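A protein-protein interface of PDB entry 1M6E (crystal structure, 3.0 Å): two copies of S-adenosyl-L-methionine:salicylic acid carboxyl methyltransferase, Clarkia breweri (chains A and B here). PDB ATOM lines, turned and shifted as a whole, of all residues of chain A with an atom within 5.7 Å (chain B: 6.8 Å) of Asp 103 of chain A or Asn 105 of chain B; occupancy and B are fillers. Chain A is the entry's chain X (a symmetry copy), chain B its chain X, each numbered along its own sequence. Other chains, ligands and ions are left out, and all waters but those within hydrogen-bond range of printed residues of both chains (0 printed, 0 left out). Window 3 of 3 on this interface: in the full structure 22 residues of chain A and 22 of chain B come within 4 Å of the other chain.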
ATOM      1  N   GLY A  12      -4.108 -12.655  -5.066  1.00  0.00           N
ATOM      2  CA  GLY A  12      -4.627 -11.294  -5.201  1.00  0.00           C
ATOM      3  C   GLY A  12      -3.998 -10.303  -6.170  1.00  0.00           C
ATOM      4  O   GLY A  12      -2.844  -9.914  -6.036  1.00  0.00           O
ATOM      5  N   ALA A  13      -4.812  -9.886  -7.139  1.00  0.00           N
ATOM      6  CA  ALA A  13      -4.464  -8.969  -8.237  1.00  0.00           C
ATOM      7  C   ALA A  13      -3.462  -7.859  -7.991  1.00  0.00           C
ATOM      8  O   ALA A  13      -3.159  -7.506  -6.845  1.00  0.00           O
ATOM      9  CB  ALA A  13      -5.754  -8.362  -8.859  1.00  0.00           C
ATOM     10  N   SER A  61     -13.436 -13.328 -10.251  1.00  0.00           N
ATOM     11  CA  SER A  61     -12.264 -13.359  -9.419  1.00  0.00           C
ATOM     12  C   SER A  61     -11.715 -11.995  -9.117  1.00  0.00           C
ATOM     13  O   SER A  61     -12.345 -11.215  -8.424  1.00  0.00           O
ATOM     14  CB  SER A  61     -11.202 -14.228 -10.041  1.00  0.00           C
ATOM     15  OG  SER A  61     -10.523 -14.887  -8.991  1.00  0.00           O
ATOM     16  N   SER A  62     -10.524 -11.716  -9.615  1.00  0.00           N
ATOM     17  CA  SER A  62      -9.913 -10.423  -9.413  1.00  0.00           C
ATOM     18  C   SER A  62      -9.421 -10.077 -10.804  1.00  0.00           C
ATOM     19  O   SER A  62      -9.376 -10.933 -11.695  1.00  0.00           O
ATOM     20  CB  SER A  62      -8.720 -10.521  -8.456  1.00  0.00           C
ATOM     21  OG  SER A  62      -9.062 -11.162  -7.242  1.00  0.00           O
ATOM     22  N   GLY A 101     -13.132 -13.301   1.065  1.00  0.00           N
ATOM     23  CA  GLY A 101     -11.700 -13.500   0.965  1.00  0.00           C
ATOM     24  C   GLY A 101     -11.148 -13.712  -0.438  1.00  0.00           C
ATOM     25  O   GLY A 101     -10.154 -14.378  -0.637  1.00  0.00           O
ATOM     26  N   ASN A 102     -11.851 -13.173  -1.419  1.00  0.00           N
ATOM     27  CA  ASN A 102     -11.403 -13.172  -2.794  1.00  0.00           C
ATOM     28  C   ASN A 102     -10.926 -11.705  -2.810  1.00  0.00           C
ATOM     29  O   ASN A 102     -11.010 -11.037  -1.788  1.00  0.00           O
ATOM     30  CB  ASN A 102     -12.586 -13.372  -3.736  1.00  0.00           C
ATOM     31  CG  ASN A 102     -12.304 -12.854  -5.141  1.00  0.00           C
ATOM     32  OD1 ASN A 102     -11.260 -13.208  -5.750  1.00  0.00           O
ATOM     33  ND2 ASN A 102     -13.218 -12.012  -5.668  1.00  0.00           N
ATOM     34  N   ASP A 103     -10.427 -11.175  -3.914  1.00  0.00           N
ATOM     35  CA  ASP A 103     -10.005  -9.784  -3.864  1.00  0.00           C
ATOM     36  C   ASP A 103     -11.047  -8.828  -4.398  1.00  0.00           C
ATOM     37  O   ASP A 103     -10.934  -8.320  -5.521  1.00  0.00           O
ATOM     38  CB  ASP A 103      -8.714  -9.584  -4.626  1.00  0.00           C
ATOM     39  CG  ASP A 103      -7.831  -8.568  -3.965  1.00  0.00           C
ATOM     40  OD1 ASP A 103      -8.386  -7.714  -3.229  1.00  0.00           O
ATOM     41  OD2 ASP A 103      -6.598  -8.623  -4.182  1.00  0.00           O
ATOM     42  N   PHE A 104     -12.079  -8.575  -3.593  1.00  0.00           N
ATOM     43  CA  PHE A 104     -13.138  -7.665  -4.016  1.00  0.00           C
ATOM     44  C   PHE A 104     -12.635  -6.246  -4.057  1.00  0.00           C
ATOM     45  O   PHE A 104     -13.027  -5.493  -4.925  1.00  0.00           O
ATOM     46  CB  PHE A 104     -14.350  -7.793  -3.109  1.00  0.00           C
ATOM     47  CG  PHE A 104     -15.162  -9.038  -3.376  1.00  0.00           C
ATOM     48  CD1 PHE A 104     -14.901 -10.211  -2.697  1.00  0.00           C
ATOM     49  CD2 PHE A 104     -16.128  -9.049  -4.375  1.00  0.00           C
ATOM     50  CE1 PHE A 104     -15.576 -11.360  -3.010  1.00  0.00           C
ATOM     51  CE2 PHE A 104     -16.810 -10.205  -4.696  1.00  0.00           C
ATOM     52  CZ  PHE A 104     -16.540 -11.358  -4.024  1.00  0.00           C
ATOM     53  N   ASN A 105     -11.730  -5.901  -3.140  1.00  0.00           N
ATOM     54  CA  ASN A 105     -11.149  -4.562  -3.087  1.00  0.00           C
ATOM     55  C   ASN A 105     -10.450  -4.268  -4.387  1.00  0.00           C
ATOM     56  O   ASN A 105     -10.607  -3.193  -4.961  1.00  0.00           O
ATOM     57  CB  ASN A 105     -10.164  -4.432  -1.915  1.00  0.00           C
ATOM     58  CG  ASN A 105     -10.869  -4.293  -0.555  1.00  0.00           C
ATOM     59  OD1 ASN A 105     -12.061  -4.589  -0.404  1.00  0.00           O
ATOM     60  ND2 ASN A 105     -10.130  -3.859   0.440  1.00  0.00           N
ATOM     61  N   ALA A 106      -9.708  -5.248  -4.876  1.00  0.00           N
ATOM     62  CA  ALA A 106      -8.959  -5.092  -6.115  1.00  0.00           C
ATOM     63  C   ALA A 106      -9.863  -4.777  -7.281  1.00  0.00           C
ATOM     64  O   ALA A 106      -9.513  -3.931  -8.122  1.00  0.00           O
ATOM     65  CB  ALA A 106      -8.178  -6.328  -6.401  1.00  0.00           C
ATOM     66  N   ILE A 107     -11.005  -5.465  -7.361  1.00  0.00           N
ATOM     67  CA  ILE A 107     -11.954  -5.164  -8.434  1.00  0.00           C
ATOM     68  C   ILE A 107     -12.606  -3.793  -8.202  1.00  0.00           C
ATOM     69  O   ILE A 107     -12.541  -2.930  -9.055  1.00  0.00           O
ATOM     70  CB  ILE A 107     -13.107  -6.141  -8.524  1.00  0.00           C
ATOM     71  CG1 ILE A 107     -12.613  -7.578  -8.397  1.00  0.00           C
ATOM     72  CG2 ILE A 107     -13.821  -5.906  -9.845  1.00  0.00           C
ATOM     73  CD1 ILE A 107     -13.758  -8.582  -8.436  1.00  0.00           C
ATOM     74  N   PHE A 108     -13.217  -3.591  -7.041  1.00  0.00           N
ATOM     75  CA  PHE A 108     -13.863  -2.334  -6.751  1.00  0.00           C
ATOM     76  C   PHE A 108     -12.943  -1.163  -7.037  1.00  0.00           C
ATOM     77  O   PHE A 108     -13.396  -0.060  -7.415  1.00  0.00           O
ATOM     78  CB  PHE A 108     -14.322  -2.321  -5.300  1.00  0.00           C
ATOM     79  CG  PHE A 108     -15.449  -3.270  -5.023  1.00  0.00           C
ATOM     80  CD1 PHE A 108     -15.830  -3.555  -3.717  1.00  0.00           C
ATOM     81  CD2 PHE A 108     -16.080  -3.956  -6.078  1.00  0.00           C
ATOM     82  CE1 PHE A 108     -16.809  -4.513  -3.466  1.00  0.00           C
ATOM     83  CE2 PHE A 108     -17.045  -4.896  -5.829  1.00  0.00           C
ATOM     84  CZ  PHE A 108     -17.414  -5.182  -4.515  1.00  0.00           C
ATOM     85  N   ASN B 102     -12.633   1.306   0.146  1.00  0.00           N
ATOM     86  CA  ASN B 102     -13.037   1.306   1.535  1.00  0.00           C
ATOM     87  C   ASN B 102     -12.596  -0.143   1.833  1.00  0.00           C
ATOM     88  O   ASN B 102     -12.065  -0.801   0.948  1.00  0.00           O
ATOM     89  CB  ASN B 102     -14.551   1.450   1.646  1.00  0.00           C
ATOM     90  CG  ASN B 102     -15.089   0.927   2.972  1.00  0.00           C
ATOM     91  OD1 ASN B 102     -14.583   1.312   4.059  1.00  0.00           O
ATOM     92  ND2 ASN B 102     -16.108   0.045   2.904  1.00  0.00           N
ATOM     93  N   ASP B 103     -12.784  -0.665   3.033  1.00  0.00           N
ATOM     94  CA  ASP B 103     -12.355  -2.039   3.245  1.00  0.00           C
ATOM     95  C   ASP B 103     -13.480  -3.040   3.112  1.00  0.00           C
ATOM     96  O   ASP B 103     -13.998  -3.557   4.110  1.00  0.00           O
ATOM     97  CB  ASP B 103     -11.710  -2.199   4.604  1.00  0.00           C
ATOM     98  CG  ASP B 103     -10.570  -3.173   4.565  1.00  0.00           C
ATOM     99  OD1 ASP B 103     -10.582  -4.039   3.654  1.00  0.00           O
ATOM    100  OD2 ASP B 103      -9.676  -3.074   5.437  1.00  0.00           O
ATOM    101  N   PHE B 104     -13.870  -3.322   1.869  1.00  0.00           N
ATOM    102  CA  PHE B 104     -14.948  -4.277   1.634  1.00  0.00           C
ATOM    103  C   PHE B 104     -14.502  -5.677   1.967  1.00  0.00           C
ATOM    104  O   PHE B 104     -15.286  -6.454   2.473  1.00  0.00           O
ATOM    105  CB  PHE B 104     -15.444  -4.184   0.201  1.00  0.00           C
ATOM    106  CG  PHE B 104     -16.312  -2.974  -0.049  1.00  0.00           C
ATOM    107  CD1 PHE B 104     -15.759  -1.784  -0.479  1.00  0.00           C
ATOM    108  CD2 PHE B 104     -17.672  -3.012   0.233  1.00  0.00           C
ATOM    109  CE1 PHE B 104     -16.537  -0.665  -0.612  1.00  0.00           C
ATOM    110  CE2 PHE B 104     -18.461  -1.886   0.101  1.00  0.00           C
ATOM    111  CZ  PHE B 104     -17.903  -0.716  -0.316  1.00  0.00           C
ATOM    112  N   ASN B 105     -13.225  -5.976   1.722  1.00  0.00           N
ATOM    113  CA  ASN B 105     -12.665  -7.291   2.020  1.00  0.00           C
ATOM    114  C   ASN B 105     -12.808  -7.574   3.491  1.00  0.00           C
ATOM    115  O   ASN B 105     -13.220  -8.661   3.890  1.00  0.00           O
ATOM    116  CB  ASN B 105     -11.187  -7.370   1.607  1.00  0.00           C
ATOM    117  CG  ASN B 105     -11.000  -7.520   0.087  1.00  0.00           C
ATOM    118  OD1 ASN B 105     -11.911  -7.267  -0.711  1.00  0.00           O
ATOM    119  ND2 ASN B 105      -9.813  -7.914  -0.314  1.00  0.00           N
ATOM    120  N   ALA B 106     -12.507  -6.572   4.302  1.00  0.00           N
ATOM    121  CA  ALA B 106     -12.579  -6.714   5.750  1.00  0.00           C
ATOM    122  C   ALA B 106     -13.970  -7.077   6.209  1.00  0.00           C
ATOM    123  O   ALA B 106     -14.122  -7.919   7.110  1.00  0.00           O
ATOM    124  CB  ALA B 106     -12.141  -5.453   6.411  1.00  0.00           C
ATOM    125  N   ILE B 107     -14.984  -6.434   5.624  1.00  0.00           N
ATOM    126  CA  ILE B 107     -16.359  -6.783   5.981  1.00  0.00           C
ATOM    127  C   ILE B 107     -16.716  -8.175   5.439  1.00  0.00           C
ATOM    128  O   ILE B 107     -17.109  -9.045   6.191  1.00  0.00           O
ATOM    129  CB  ILE B 107     -17.400  -5.851   5.397  1.00  0.00           C
ATOM    130  CG1 ILE B 107     -16.975  -4.395   5.552  1.00  0.00           C
ATOM    131  CG2 ILE B 107     -18.724  -6.129   6.089  1.00  0.00           C
ATOM    132  CD1 ILE B 107     -17.981  -3.436   4.928  1.00  0.00           C
ATOM    133  N   PHE B 108     -16.560  -8.386   4.138  1.00  0.00           N
ATOM    134  CA  PHE B 108     -16.883  -9.664   3.549  1.00  0.00           C
ATOM    135  C   PHE B 108     -16.239 -10.801   4.317  1.00  0.00           C
ATOM    136  O   PHE B 108     -16.785 -11.926   4.388  1.00  0.00           O
ATOM    137  CB  PHE B 108     -16.446  -9.677   2.091  1.00  0.00           C
ATOM    138  CG  PHE B 108     -17.257  -8.768   1.218  1.00  0.00           C
ATOM    139  CD1 PHE B 108     -16.848  -8.483  -0.080  1.00  0.00           C
ATOM    140  CD2 PHE B 108     -18.398  -8.118   1.727  1.00  0.00           C
ATOM    141  CE1 PHE B 108     -17.552  -7.559  -0.849  1.00  0.00           C
ATOM    142  CE2 PHE B 108     -19.091  -7.213   0.968  1.00  0.00           C
ATOM    143  CZ  PHE B 108     -18.667  -6.926  -0.329  1.00  0.00           C
ATOM    144  N   ARG B 109     -15.082 -10.511   4.909  1.00  0.00           N
ATOM    145  CA  ARG B 109     -14.371 -11.527   5.661  1.00  0.00           C
ATOM    146  C   ARG B 109     -14.724 -11.537   7.152  1.00  0.00           C
ATOM    147  O   ARG B 109     -15.740 -12.083   7.565  1.00  0.00           O
ATOM    148  CB  ARG B 109     -12.871 -11.343   5.484  1.00  0.00           C
ATOM    149  CG  ARG B 109     -12.345 -11.411   4.054  1.00  0.00           C
ATOM    150  CD  ARG B 109     -10.923 -11.977   4.035  1.00  0.00           C
ATOM    151  NE  ARG B 109      -9.862 -11.137   3.462  1.00  0.00           N
ATOM    152  CZ  ARG B 109      -9.847 -10.651   2.219  1.00  0.00           C
ATOM    153  NH1 ARG B 109     -10.852 -10.880   1.380  1.00  0.00           N
ATOM    154  NH2 ARG B 109      -8.774  -9.993   1.785  1.00  0.00           N
ATOM    155  N   SER B 110     -13.887 -10.902   7.961  1.00  0.00           N
ATOM    156  CA  SER B 110     -14.100 -10.882   9.400  1.00  0.00           C
ATOM    157  C   SER B 110     -15.521 -10.539   9.833  1.00  0.00           C
ATOM    158  O   SER B 110     -15.828 -10.596  11.023  1.00  0.00           O
ATOM    159  CB  SER B 110     -13.098  -9.934  10.082  1.00  0.00           C
ATOM    160  OG  SER B 110     -12.887 -10.315  11.440  1.00  0.00           O
ATOM    161  N   LEU B 111     -16.399 -10.173   8.908  1.00  0.00           N
ATOM    162  CA  LEU B 111     -17.755  -9.890   9.346  1.00  0.00           C
ATOM    163  C   LEU B 111     -18.764 -10.960   8.886  1.00  0.00           C
ATOM    164  O   LEU B 111     -19.081 -11.842   9.687  1.00  0.00           O
ATOM    165  CB  LEU B 111     -18.171  -8.448   8.976  1.00  0.00           C
ATOM    166  CG  LEU B 111     -18.010  -7.392  10.097  1.00  0.00           C
ATOM    167  CD1 LEU B 111     -17.922  -5.998   9.505  1.00  0.00           C
ATOM    168  CD2 LEU B 111     -19.179  -7.497  11.093  1.00  0.00           C
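Asp 103 of chain A touches Asn 105 of chain B, and with the chains exchanged Asn 105 of chain A touches Asp 103 of chain B.
Phe 104 of chain A touches Asn 105 of chain B, and with the chains exchanged Asn 105 of chain A touches Phe 104 of chain B.
Phe 104 of chain A touches Phe 108 of chain B, and with the chains exchanged Phe 108 of chain A touches Phe 104 of chain B.
Asn 105 of chain A touches its own counterpart, Asn 105 of chain B.
Positions printed for both chains: 102, 103, 104, 105, 106, 107 and 108.
Of the 11 pairs that touch across the chains among the printed residues, 9 have their exchanged pair printed and touching as well.
Among the printed residues, pairs that only touch across the chains: Asn 105 of chain A with Asn 102 of chain B (3.7 Å), Asn 102 of chain A with Asn 105 of chain B (3.7 Å), Phe 104 of chain A with Phe 108 of chain B (3.7 Å) and Phe 108 of chain A with Phe 104 of chain B (3.7 Å).
The guanidinium group (NH1) of Arg 109 of chain B sits close to the backbone NH (N) of Gly 101 of chain A (3.3 Å).
The side-chain amide oxygen (OD1) of Asn 105 of chain A lies close to the side-chain amide oxygen (OD1) of Asn 105 of chain B, at 2.7 Å.
OD1 of Asn 105 of chain A sits at hydrogen-bond distance from N of Phe 104 of chain B, 3.2 Å away.
The guanidinium group (NH1) of Arg 109 of chain B lies within hydrogen-bond range of the backbone carbonyl oxygen (O) of Asn 102 of chain A (3.2 Å).
The side-chain amide nitrogen (ND2) of Asn 105 of chain B sits at hydrogen-bond distance from the side-chain carboxylate (OD1) of Asp 103 of chain A, at 3.3 Å.
The side-chain carboxylate (OD1) of Asp 103 of chain B lies within hydrogen-bond range of the side-chain amide nitrogen (ND2) of Asn 105 of chain A (3.3 Å).
The side-chain amide oxygen (OD1) of Asn 105 of chain B lies within hydrogen-bond range of the backbone NH (N) of Phe 104 of chain A (3.2 Å).
Asp 103 of chain A touches just one residue of chain B: Asn 105 (3.3 Å).
Printed residues of chain B within 4 Å of Phe 108 of chain A: Phe 104.
Of the printed residues of chain A, Asp 103 of chain B touches Asn 105 (3.3 Å).
Of the printed residues of chain A, Asn 105 of chain B touches Asn 102 (3.7 Å), Asp 103 (3.3 Å), Phe 104 (3.2 Å) and Asn 105 (2.7 Å).
The nearest residue of chain B that does not touch Asp 103 of chain A is Arg 109 of chain B (5.3 Å).
The nearest residue of chain A that does not touch Asn 105 of chain B is Ala 106 of chain A (5.1 Å).
Hydrophobic or aromatic side chains of chain B that line the printed part of chain A: Phe 104 and Phe 108.
Printed residues of chain A that touch a printed residue of chain B: Gly 101, Asn 102, Asp 103, Phe 104, Asn 105 and Phe 108.
Hydrophobic or aromatic side chains of chain A that line the printed part of chain B: Phe 104 and Phe 108.
The backbone carbonyl oxygen (O) of Ser 61 of chain A sits at hydrogen-bond distance from the side-chain amide nitrogen (ND2) of Asn 102 of chain A (3.0 Å).
The backbone NH (N) of Ala 106 of chain A is in hydrogen-bond range of the side-chain carboxylate (OD1) of Asp 103 of chain A, 3.2 Å away.
The side-chain amide oxygen (OD1) of Asn 102 of chain A is in hydrogen-bond range of the side-chain hydroxyl (OG) of Ser 62 of chain A (3.4 Å).
NH2 of Arg 109 of chain B lies close to ND2 of Asn 105 of chain B, 3.1 Å away.
The side-chain carboxylate (OD1) of Asp 103 of chain B lies within hydrogen-bond range of the backbone NH (N) of Ala 106 of chain B, at 3.2 Å.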
